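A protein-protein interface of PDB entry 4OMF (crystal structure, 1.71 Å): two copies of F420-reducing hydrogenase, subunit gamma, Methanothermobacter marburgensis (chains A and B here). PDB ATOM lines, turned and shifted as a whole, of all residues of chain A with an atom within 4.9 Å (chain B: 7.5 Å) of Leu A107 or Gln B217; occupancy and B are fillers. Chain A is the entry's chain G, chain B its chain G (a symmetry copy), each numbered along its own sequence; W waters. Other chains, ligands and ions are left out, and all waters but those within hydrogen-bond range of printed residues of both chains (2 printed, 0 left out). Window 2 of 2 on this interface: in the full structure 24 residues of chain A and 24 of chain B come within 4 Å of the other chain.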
ATOM      1  N   VAL A 105     -11.987 -10.018  24.203  1.00  0.00           N
ATOM      2  CA  VAL A 105     -11.989 -11.378  23.700  1.00  0.00           C
ATOM      3  C   VAL A 105     -13.425 -11.864  23.539  1.00  0.00           C
ATOM      4  O   VAL A 105     -14.276 -11.639  24.396  1.00  0.00           O
ATOM      5  CB  VAL A 105     -11.159 -12.318  24.630  1.00  0.00           C
ATOM      6  CG1 VAL A 105     -11.732 -12.364  26.046  1.00  0.00           C
ATOM      7  CG2 VAL A 105     -11.023 -13.735  24.019  1.00  0.00           C
ATOM      8  N   CYS A 106     -13.687 -12.521  22.417  1.00  0.00           N
ATOM      9  CA  CYS A 106     -15.016 -13.029  22.089  1.00  0.00           C
ATOM     10  C   CYS A 106     -15.191 -14.419  22.676  1.00  0.00           C
ATOM     11  O   CYS A 106     -14.420 -15.316  22.352  1.00  0.00           O
ATOM     12  CB  CYS A 106     -15.207 -13.073  20.574  1.00  0.00           C
ATOM     13  SG  CYS A 106     -16.788 -13.779  20.096  1.00  0.00           S
ATOM     14  N   LEU A 107     -16.199 -14.590  23.531  1.00  0.00           N
ATOM     15  CA  LEU A 107     -16.388 -15.863  24.247  1.00  0.00           C
ATOM     16  C   LEU A 107     -16.784 -16.986  23.287  1.00  0.00           C
ATOM     17  O   LEU A 107     -16.596 -18.191  23.574  1.00  0.00           O
ATOM     18  CB  LEU A 107     -17.455 -15.709  25.341  1.00  0.00           C
ATOM     19  CG  LEU A 107     -17.138 -14.707  26.448  1.00  0.00           C
ATOM     20  CD1 LEU A 107     -18.236 -14.734  27.515  1.00  0.00           C
ATOM     21  CD2 LEU A 107     -15.781 -15.030  27.074  1.00  0.00           C
ATOM     22  N   GLN A 108     -17.316 -16.597  22.134  1.00  0.00           N
ATOM     23  CA  GLN A 108     -17.707 -17.575  21.125  1.00  0.00           C
ATOM     24  C   GLN A 108     -16.629 -17.846  20.058  1.00  0.00           C
ATOM     25  O   GLN A 108     -16.920 -18.480  19.041  1.00  0.00           O
ATOM     26  CB  GLN A 108     -19.015 -17.136  20.432  1.00  0.00           C
ATOM     27  CG  GLN A 108     -20.257 -17.155  21.353  1.00  0.00           C
ATOM     28  CD  GLN A 108     -20.494 -15.836  22.110  1.00  0.00           C
ATOM     29  OE1 GLN A 108     -20.154 -14.762  21.633  1.00  0.00           O
ATOM     30  NE2 GLN A 108     -21.081 -15.931  23.301  1.00  0.00           N
ATOM     31  N   ASP A 109     -15.390 -17.394  20.277  1.00  0.00           N
ATOM     32  CA  ASP A 109     -14.316 -17.710  19.313  1.00  0.00           C
ATOM     33  C   ASP A 109     -13.223 -18.534  19.949  1.00  0.00           C
ATOM     34  O   ASP A 109     -12.420 -18.027  20.728  1.00  0.00           O
ATOM     35  CB  ASP A 109     -13.682 -16.451  18.700  1.00  0.00           C
ATOM     36  CG  ASP A 109     -12.797 -16.800  17.504  1.00  0.00           C
ATOM     37  OD1 ASP A 109     -13.296 -17.506  16.593  1.00  0.00           O
ATOM     38  OD2 ASP A 109     -11.601 -16.436  17.501  1.00  0.00           O
ATOM     39  N   LEU A 113      -9.726 -17.503  22.420  1.00  0.00           N
ATOM     40  CA  LEU A 113      -9.604 -17.959  23.803  1.00  0.00           C
ATOM     41  C   LEU A 113      -8.311 -18.724  24.018  1.00  0.00           C
ATOM     42  O   LEU A 113      -7.660 -18.548  25.048  1.00  0.00           O
ATOM     43  CB  LEU A 113     -10.787 -18.837  24.202  1.00  0.00           C
ATOM     44  CG  LEU A 113     -12.126 -18.098  24.311  1.00  0.00           C
ATOM     45  CD1 LEU A 113     -13.273 -19.108  24.391  1.00  0.00           C
ATOM     46  CD2 LEU A 113     -12.122 -17.161  25.507  1.00  0.00           C
ATOM     47  N   ARG A 140     -18.400  -3.467  24.698  1.00  0.00           N
ATOM     48  CA  ARG A 140     -19.396  -3.673  25.745  1.00  0.00           C
ATOM     49  C   ARG A 140     -20.820  -3.602  25.138  1.00  0.00           C
ATOM     50  O   ARG A 140     -21.731  -4.241  25.661  1.00  0.00           O
ATOM     51  CB  ARG A 140     -19.266  -2.620  26.854  1.00  0.00           C
ATOM     52  CG  ARG A 140     -18.076  -2.815  27.809  1.00  0.00           C
ATOM     53  CD  ARG A 140     -18.271  -4.103  28.589  1.00  0.00           C
ATOM     54  NE  ARG A 140     -17.264  -4.236  29.657  1.00  0.00           N
ATOM     55  CZ  ARG A 140     -17.176  -5.250  30.509  1.00  0.00           C
ATOM     56  NH1 ARG A 140     -18.032  -6.271  30.465  1.00  0.00           N
ATOM     57  NH2 ARG A 140     -16.215  -5.241  31.432  1.00  0.00           N
ATOM     58  N   SER A 154     -20.597 -12.116  22.480  1.00  0.00           N
ATOM     59  CA  SER A 154     -20.143 -11.780  23.823  1.00  0.00           C
ATOM     60  C   SER A 154     -18.664 -11.402  23.880  1.00  0.00           C
ATOM     61  O   SER A 154     -17.816 -12.237  23.600  1.00  0.00           O
ATOM     62  CB  SER A 154     -20.394 -12.980  24.757  1.00  0.00           C
ATOM     63  OG  SER A 154     -21.737 -13.428  24.659  1.00  0.00           O
ATOM     64  N   VAL A 156     -15.517  -9.616  26.280  1.00  0.00           N
ATOM     65  CA  VAL A 156     -15.149  -9.210  27.647  1.00  0.00           C
ATOM     66  C   VAL A 156     -13.696  -8.712  27.680  1.00  0.00           C
ATOM     67  O   VAL A 156     -12.893  -9.136  26.842  1.00  0.00           O
ATOM     68  CB  VAL A 156     -15.338 -10.365  28.668  1.00  0.00           C
ATOM     69  CG1 VAL A 156     -16.831 -10.703  28.835  1.00  0.00           C
ATOM     70  CG2 VAL A 156     -14.517 -11.611  28.304  1.00  0.00           C
ATOM     71  N   ASP A 160     -11.146 -10.702  32.562  1.00  0.00           N
ATOM     72  CA  ASP A 160     -12.253 -11.597  32.899  1.00  0.00           C
ATOM     73  C   ASP A 160     -11.869 -13.064  32.702  1.00  0.00           C
ATOM     74  O   ASP A 160     -12.532 -13.959  33.232  1.00  0.00           O
ATOM     75  CB  ASP A 160     -13.491 -11.283  32.059  1.00  0.00           C
ATOM     76  CG  ASP A 160     -14.313 -10.100  32.605  1.00  0.00           C
ATOM     77  OD1 ASP A 160     -13.805  -9.293  33.422  1.00  0.00           O
ATOM     78  OD2 ASP A 160     -15.495  -9.987  32.221  1.00  0.00           O
ATOM     79  N   LEU A 161     -10.809 -13.327  31.938  1.00  0.00           N
ATOM     80  CA  LEU A 161     -10.399 -14.702  31.714  1.00  0.00           C
ATOM     81  C   LEU A 161      -8.973 -15.022  32.196  1.00  0.00           C
ATOM     82  O   LEU A 161      -8.684 -16.174  32.467  1.00  0.00           O
ATOM     83  CB  LEU A 161     -10.539 -15.051  30.223  1.00  0.00           C
ATOM     84  CG  LEU A 161     -11.983 -14.889  29.735  1.00  0.00           C
ATOM     85  CD1 LEU A 161     -12.042 -15.029  28.247  1.00  0.00           C
ATOM     86  CD2 LEU A 161     -12.908 -15.906  30.415  1.00  0.00           C
ATOM     87  N   ASP B 209     -25.799  -2.775  33.017  1.00  0.00           N
ATOM     88  CA  ASP B 209     -25.530  -4.045  33.663  1.00  0.00           C
ATOM     89  C   ASP B 209     -26.042  -5.196  32.806  1.00  0.00           C
ATOM     90  O   ASP B 209     -25.516  -6.301  32.899  1.00  0.00           O
ATOM     91  CB  ASP B 209     -26.170  -4.131  35.061  1.00  0.00           C
ATOM     92  CG  ASP B 209     -25.482  -3.251  36.076  1.00  0.00           C
ATOM     93  OD1 ASP B 209     -24.356  -2.778  35.793  1.00  0.00           O
ATOM     94  OD2 ASP B 209     -26.080  -3.042  37.155  1.00  0.00           O
ATOM     95  N   LEU B 210     -27.075  -4.966  31.992  1.00  0.00           N
ATOM     96  CA  LEU B 210     -27.584  -6.069  31.169  1.00  0.00           C
ATOM     97  C   LEU B 210     -26.521  -6.480  30.150  1.00  0.00           C
ATOM     98  O   LEU B 210     -26.400  -7.659  29.800  1.00  0.00           O
ATOM     99  CB  LEU B 210     -28.894  -5.681  30.457  1.00  0.00           C
ATOM    100  CG  LEU B 210     -30.068  -5.284  31.372  1.00  0.00           C
ATOM    101  CD1 LEU B 210     -31.274  -4.885  30.525  1.00  0.00           C
ATOM    102  CD2 LEU B 210     -30.466  -6.390  32.372  1.00  0.00           C
ATOM    103  N   GLN B 211     -25.753  -5.511  29.656  1.00  0.00           N
ATOM    104  CA  GLN B 211     -24.625  -5.850  28.806  1.00  0.00           C
ATOM    105  C   GLN B 211     -23.490  -6.472  29.626  1.00  0.00           C
ATOM    106  O   GLN B 211     -23.053  -7.574  29.334  1.00  0.00           O
ATOM    107  CB  GLN B 211     -24.106  -4.614  28.055  1.00  0.00           C
ATOM    108  CG  GLN B 211     -25.082  -4.062  26.989  1.00  0.00           C
ATOM    109  CD  GLN B 211     -25.243  -5.038  25.825  1.00  0.00           C
ATOM    110  OE1 GLN B 211     -24.274  -5.401  25.125  1.00  0.00           O
ATOM    111  NE2 GLN B 211     -26.445  -5.478  25.624  1.00  0.00           N
ATOM    112  N   THR B 212     -23.017  -5.762  30.646  1.00  0.00           N
ATOM    113  CA  THR B 212     -21.762  -6.149  31.267  1.00  0.00           C
ATOM    114  C   THR B 212     -21.905  -7.463  32.037  1.00  0.00           C
ATOM    115  O   THR B 212     -20.947  -8.221  32.126  1.00  0.00           O
ATOM    116  CB  THR B 212     -21.237  -5.056  32.215  1.00  0.00           C
ATOM    117  OG1 THR B 212     -22.140  -4.918  33.311  1.00  0.00           O
ATOM    118  CG2 THR B 212     -21.135  -3.714  31.493  1.00  0.00           C
ATOM    119  N   LYS B 213     -23.096  -7.742  32.569  1.00  0.00           N
ATOM    120  CA  LYS B 213     -23.297  -8.922  33.411  1.00  0.00           C
ATOM    121  C   LYS B 213     -24.073 -10.060  32.737  1.00  0.00           C
ATOM    122  O   LYS B 213     -24.147 -11.163  33.287  1.00  0.00           O
ATOM    123  CB  LYS B 213     -24.030  -8.514  34.699  1.00  0.00           C
ATOM    124  CG  LYS B 213     -23.272  -7.440  35.480  1.00  0.00           C
ATOM    125  CD  LYS B 213     -23.955  -7.041  36.792  1.00  0.00           C
ATOM    126  CE  LYS B 213     -23.015  -6.120  37.575  1.00  0.00           C
ATOM    127  NZ  LYS B 213     -23.652  -5.610  38.804  1.00  0.00           N
ATOM    128  N   VAL B 214     -24.658  -9.802  31.568  1.00  0.00           N
ATOM    129  CA  VAL B 214     -25.459 -10.838  30.934  1.00  0.00           C
ATOM    130  C   VAL B 214     -25.045 -11.032  29.479  1.00  0.00           C
ATOM    131  O   VAL B 214     -24.475 -12.060  29.136  1.00  0.00           O
ATOM    132  CB  VAL B 214     -26.986 -10.539  30.998  1.00  0.00           C
ATOM    133  CG1 VAL B 214     -27.774 -11.776  30.549  1.00  0.00           C
ATOM    134  CG2 VAL B 214     -27.408 -10.126  32.415  1.00  0.00           C
ATOM    135  N   VAL B 215     -25.340 -10.052  28.626  1.00  0.00           N
ATOM    136  CA  VAL B 215     -25.008 -10.200  27.201  1.00  0.00           C
ATOM    137  C   VAL B 215     -23.522 -10.458  26.972  1.00  0.00           C
ATOM    138  O   VAL B 215     -23.176 -11.393  26.250  1.00  0.00           O
ATOM    139  CB  VAL B 215     -25.454  -8.977  26.399  1.00  0.00           C
ATOM    140  CG1 VAL B 215     -25.081  -9.171  24.918  1.00  0.00           C
ATOM    141  CG2 VAL B 215     -26.997  -8.774  26.568  1.00  0.00           C
ATOM    142  N   ASN B 216     -22.651  -9.654  27.582  1.00  0.00           N
ATOM    143  CA  ASN B 216     -21.191  -9.830  27.458  1.00  0.00           C
ATOM    144  C   ASN B 216     -20.673 -11.197  27.960  1.00  0.00           C
ATOM    145  O   ASN B 216     -19.589 -11.632  27.589  1.00  0.00           O
ATOM    146  CB  ASN B 216     -20.410  -8.769  28.260  1.00  0.00           C
ATOM    147  CG  ASN B 216     -20.615  -7.314  27.795  1.00  0.00           C
ATOM    148  OD1 ASN B 216     -20.228  -6.410  28.527  1.00  0.00           O
ATOM    149  ND2 ASN B 216     -21.203  -7.081  26.618  1.00  0.00           N
ATOM    150  N   GLN B 217     -21.444 -11.819  28.859  1.00  0.00           N
ATOM    151  CA  GLN B 217     -21.046 -13.045  29.553  1.00  0.00           C
ATOM    152  C   GLN B 217     -21.592 -14.293  28.866  1.00  0.00           C
ATOM    153  O   GLN B 217     -21.366 -15.405  29.334  1.00  0.00           O
ATOM    154  CB  GLN B 217     -21.544 -13.019  31.000  1.00  0.00           C
ATOM    155  CG  GLN B 217     -21.089 -11.791  31.805  1.00  0.00           C
ATOM    156  CD  GLN B 217     -19.571 -11.691  31.887  1.00  0.00           C
ATOM    157  OE1 GLN B 217     -18.868 -12.701  31.957  1.00  0.00           O
ATOM    158  NE2 GLN B 217     -19.060 -10.471  31.863  1.00  0.00           N
ATOM    159  N   GLY B 218     -22.330 -14.101  27.773  1.00  0.00           N
ATOM    160  CA  GLY B 218     -22.856 -15.219  27.008  1.00  0.00           C
ATOM    161  C   GLY B 218     -24.100 -15.824  27.633  1.00  0.00           C
ATOM    162  O   GLY B 218     -24.413 -16.998  27.427  1.00  0.00           O
ATOM    163  N   LEU B 219     -24.801 -15.015  28.407  1.00  0.00           N
ATOM    164  CA  LEU B 219     -25.933 -15.507  29.158  1.00  0.00           C
ATOM    165  C   LEU B 219     -27.289 -15.045  28.630  1.00  0.00           C
ATOM    166  O   LEU B 219     -28.312 -15.619  29.010  1.00  0.00           O
ATOM    167  CB  LEU B 219     -25.808 -15.080  30.623  1.00  0.00           C
ATOM    168  CG  LEU B 219     -24.664 -15.631  31.461  1.00  0.00           C
ATOM    169  CD1 LEU B 219     -24.641 -14.911  32.816  1.00  0.00           C
ATOM    170  CD2 LEU B 219     -24.798 -17.121  31.654  1.00  0.00           C
ATOM    171  N   CYS B 220     -27.329 -14.011  27.796  1.00  0.00           N
ATOM    172  CA  CYS B 220     -28.633 -13.476  27.409  1.00  0.00           C
ATOM    173  C   CYS B 220     -29.346 -14.416  26.456  1.00  0.00           C
ATOM    174  O   CYS B 220     -28.728 -14.939  25.512  1.00  0.00           O
ATOM    175  CB  CYS B 220     -28.496 -12.089  26.762  1.00  0.00           C
ATOM    176  SG  CYS B 220     -30.094 -11.337  26.346  1.00  0.00           S
HETATM  177  O   HOH W   1     -16.710 -12.185  33.490  1.00  0.00           O
HETATM  178  O   HOH W   2     -17.231  -8.004  32.490  1.00  0.00           O
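O of Arg A140 lies close to OE1 of Gln B211 (2.8 Å). The side-chain amide oxygen of Asn B216 sits at hydrogen-bond distance from the guanidinium group of Arg A140, at 2.9 Å. The backbone carbonyl oxygen of Val B215 sits at hydrogen-bond distance from the side-chain hydroxyl of Ser A154 (3.0 Å). The backbone NH (N) of Gly B218 sits close to the side-chain hydroxyl (OG) of Ser A154.
The backbone NH (N) of Val A105 lies within hydrogen-bond range of the backbone carbonyl oxygen (O) of Val A156 (2.9 Å). N of Leu A107 lies within hydrogen-bond range of O of Ser A154, 2.9 Å away. OE1 of Gln A108 is in hydrogen-bond range of N of Ser A154 (2.8 Å). O of Leu B210 lies within hydrogen-bond range of N of Val B215, at 2.9 Å. The backbone carbonyl oxygen of Gln B211 sits at hydrogen-bond distance from the backbone NH of Asn B216 (2.7 Å). The backbone carbonyl oxygen of Thr B212 sits at hydrogen-bond distance from the side-chain amide nitrogen of Gln B217 (2.9 Å).
CD1 of Leu A107 touches O of Asn B216, at 3.4 Å. Leu A107 touches Gln B217 (CD1 to C, 3.6 Å). Thr B212 touches Arg A140 (CA to NH1, 3.8 Å). Ser A154 touches Asn B216 (CB to O, 3.2 Å). Asn B216 touches Val A156. Gln B217 touches Val A156. OD2 of Asp A160 touches NE2 of Gln B217 (3.6 Å).
Leu A107 touches just these residues of chain B: Asn B216 and Gln B217. Gln B217 touches three residues of chain A. Printed residues of chain B within 4 Å of Val A156: Asn B216 (3.2 Å) and Gln B217 (3.8 Å). Printed residues of chain B within 4 Å of Arg A140: Gln B211 (2.8 Å), Thr B212 (3.8 Å) and Asn B216 (2.9 Å). Of the printed residues of chain A, Gln B211 touches Arg A140 (2.8 Å). Of the printed residues of chain B, Ser A154 touches Val B215, Asn B216 and Gly B218. Cys A106 touches none of the printed residues of chain B. The nearest residue of chain B that does not touch Leu A107 is Gly B218 (4.2 Å). The nearest residue of chain A that does not touch Gln B217 is Ser A154 (4.3 Å). The nearest printed residue of chain A that does not touch Gln B211 is Val A156 (7.0 Å).
Of the 11 printed residues of chain A, 5 touch a printed residue of chain B. Printed residues of chain A that touch a printed residue of chain B: Leu A107, Arg A140, Ser A154, Val A156 and Asp A160. Hydrophobic or aromatic side chains of chain A that line the printed part of chain B: Leu A107 and Val A156. Along chain B the printed residues that touch a printed residue of chain A span positions 211 to 218. Among the printed residues, no Asp or Glu carboxylate lies within 4 Å of a Lys or Arg side-chain nitrogen of the other chain.
No position is printed for both chains. Of the 11 pairs that touch across the chains among the printed residues, none has its exchanged pair printed and touching as well.
Water W2 lies within hydrogen-bond range of the side-chain carboxylate of Asp A160 (2.6 Å), the guanidinium group of Arg A140 (2.8 Å) and the side-chain amide nitrogen of Gln B217 (3.1 Å). Water W1 lies within hydrogen-bond range of OE1 of Gln B217 (2.7 Å) and OD2 of Asp A160 (2.8 Å).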
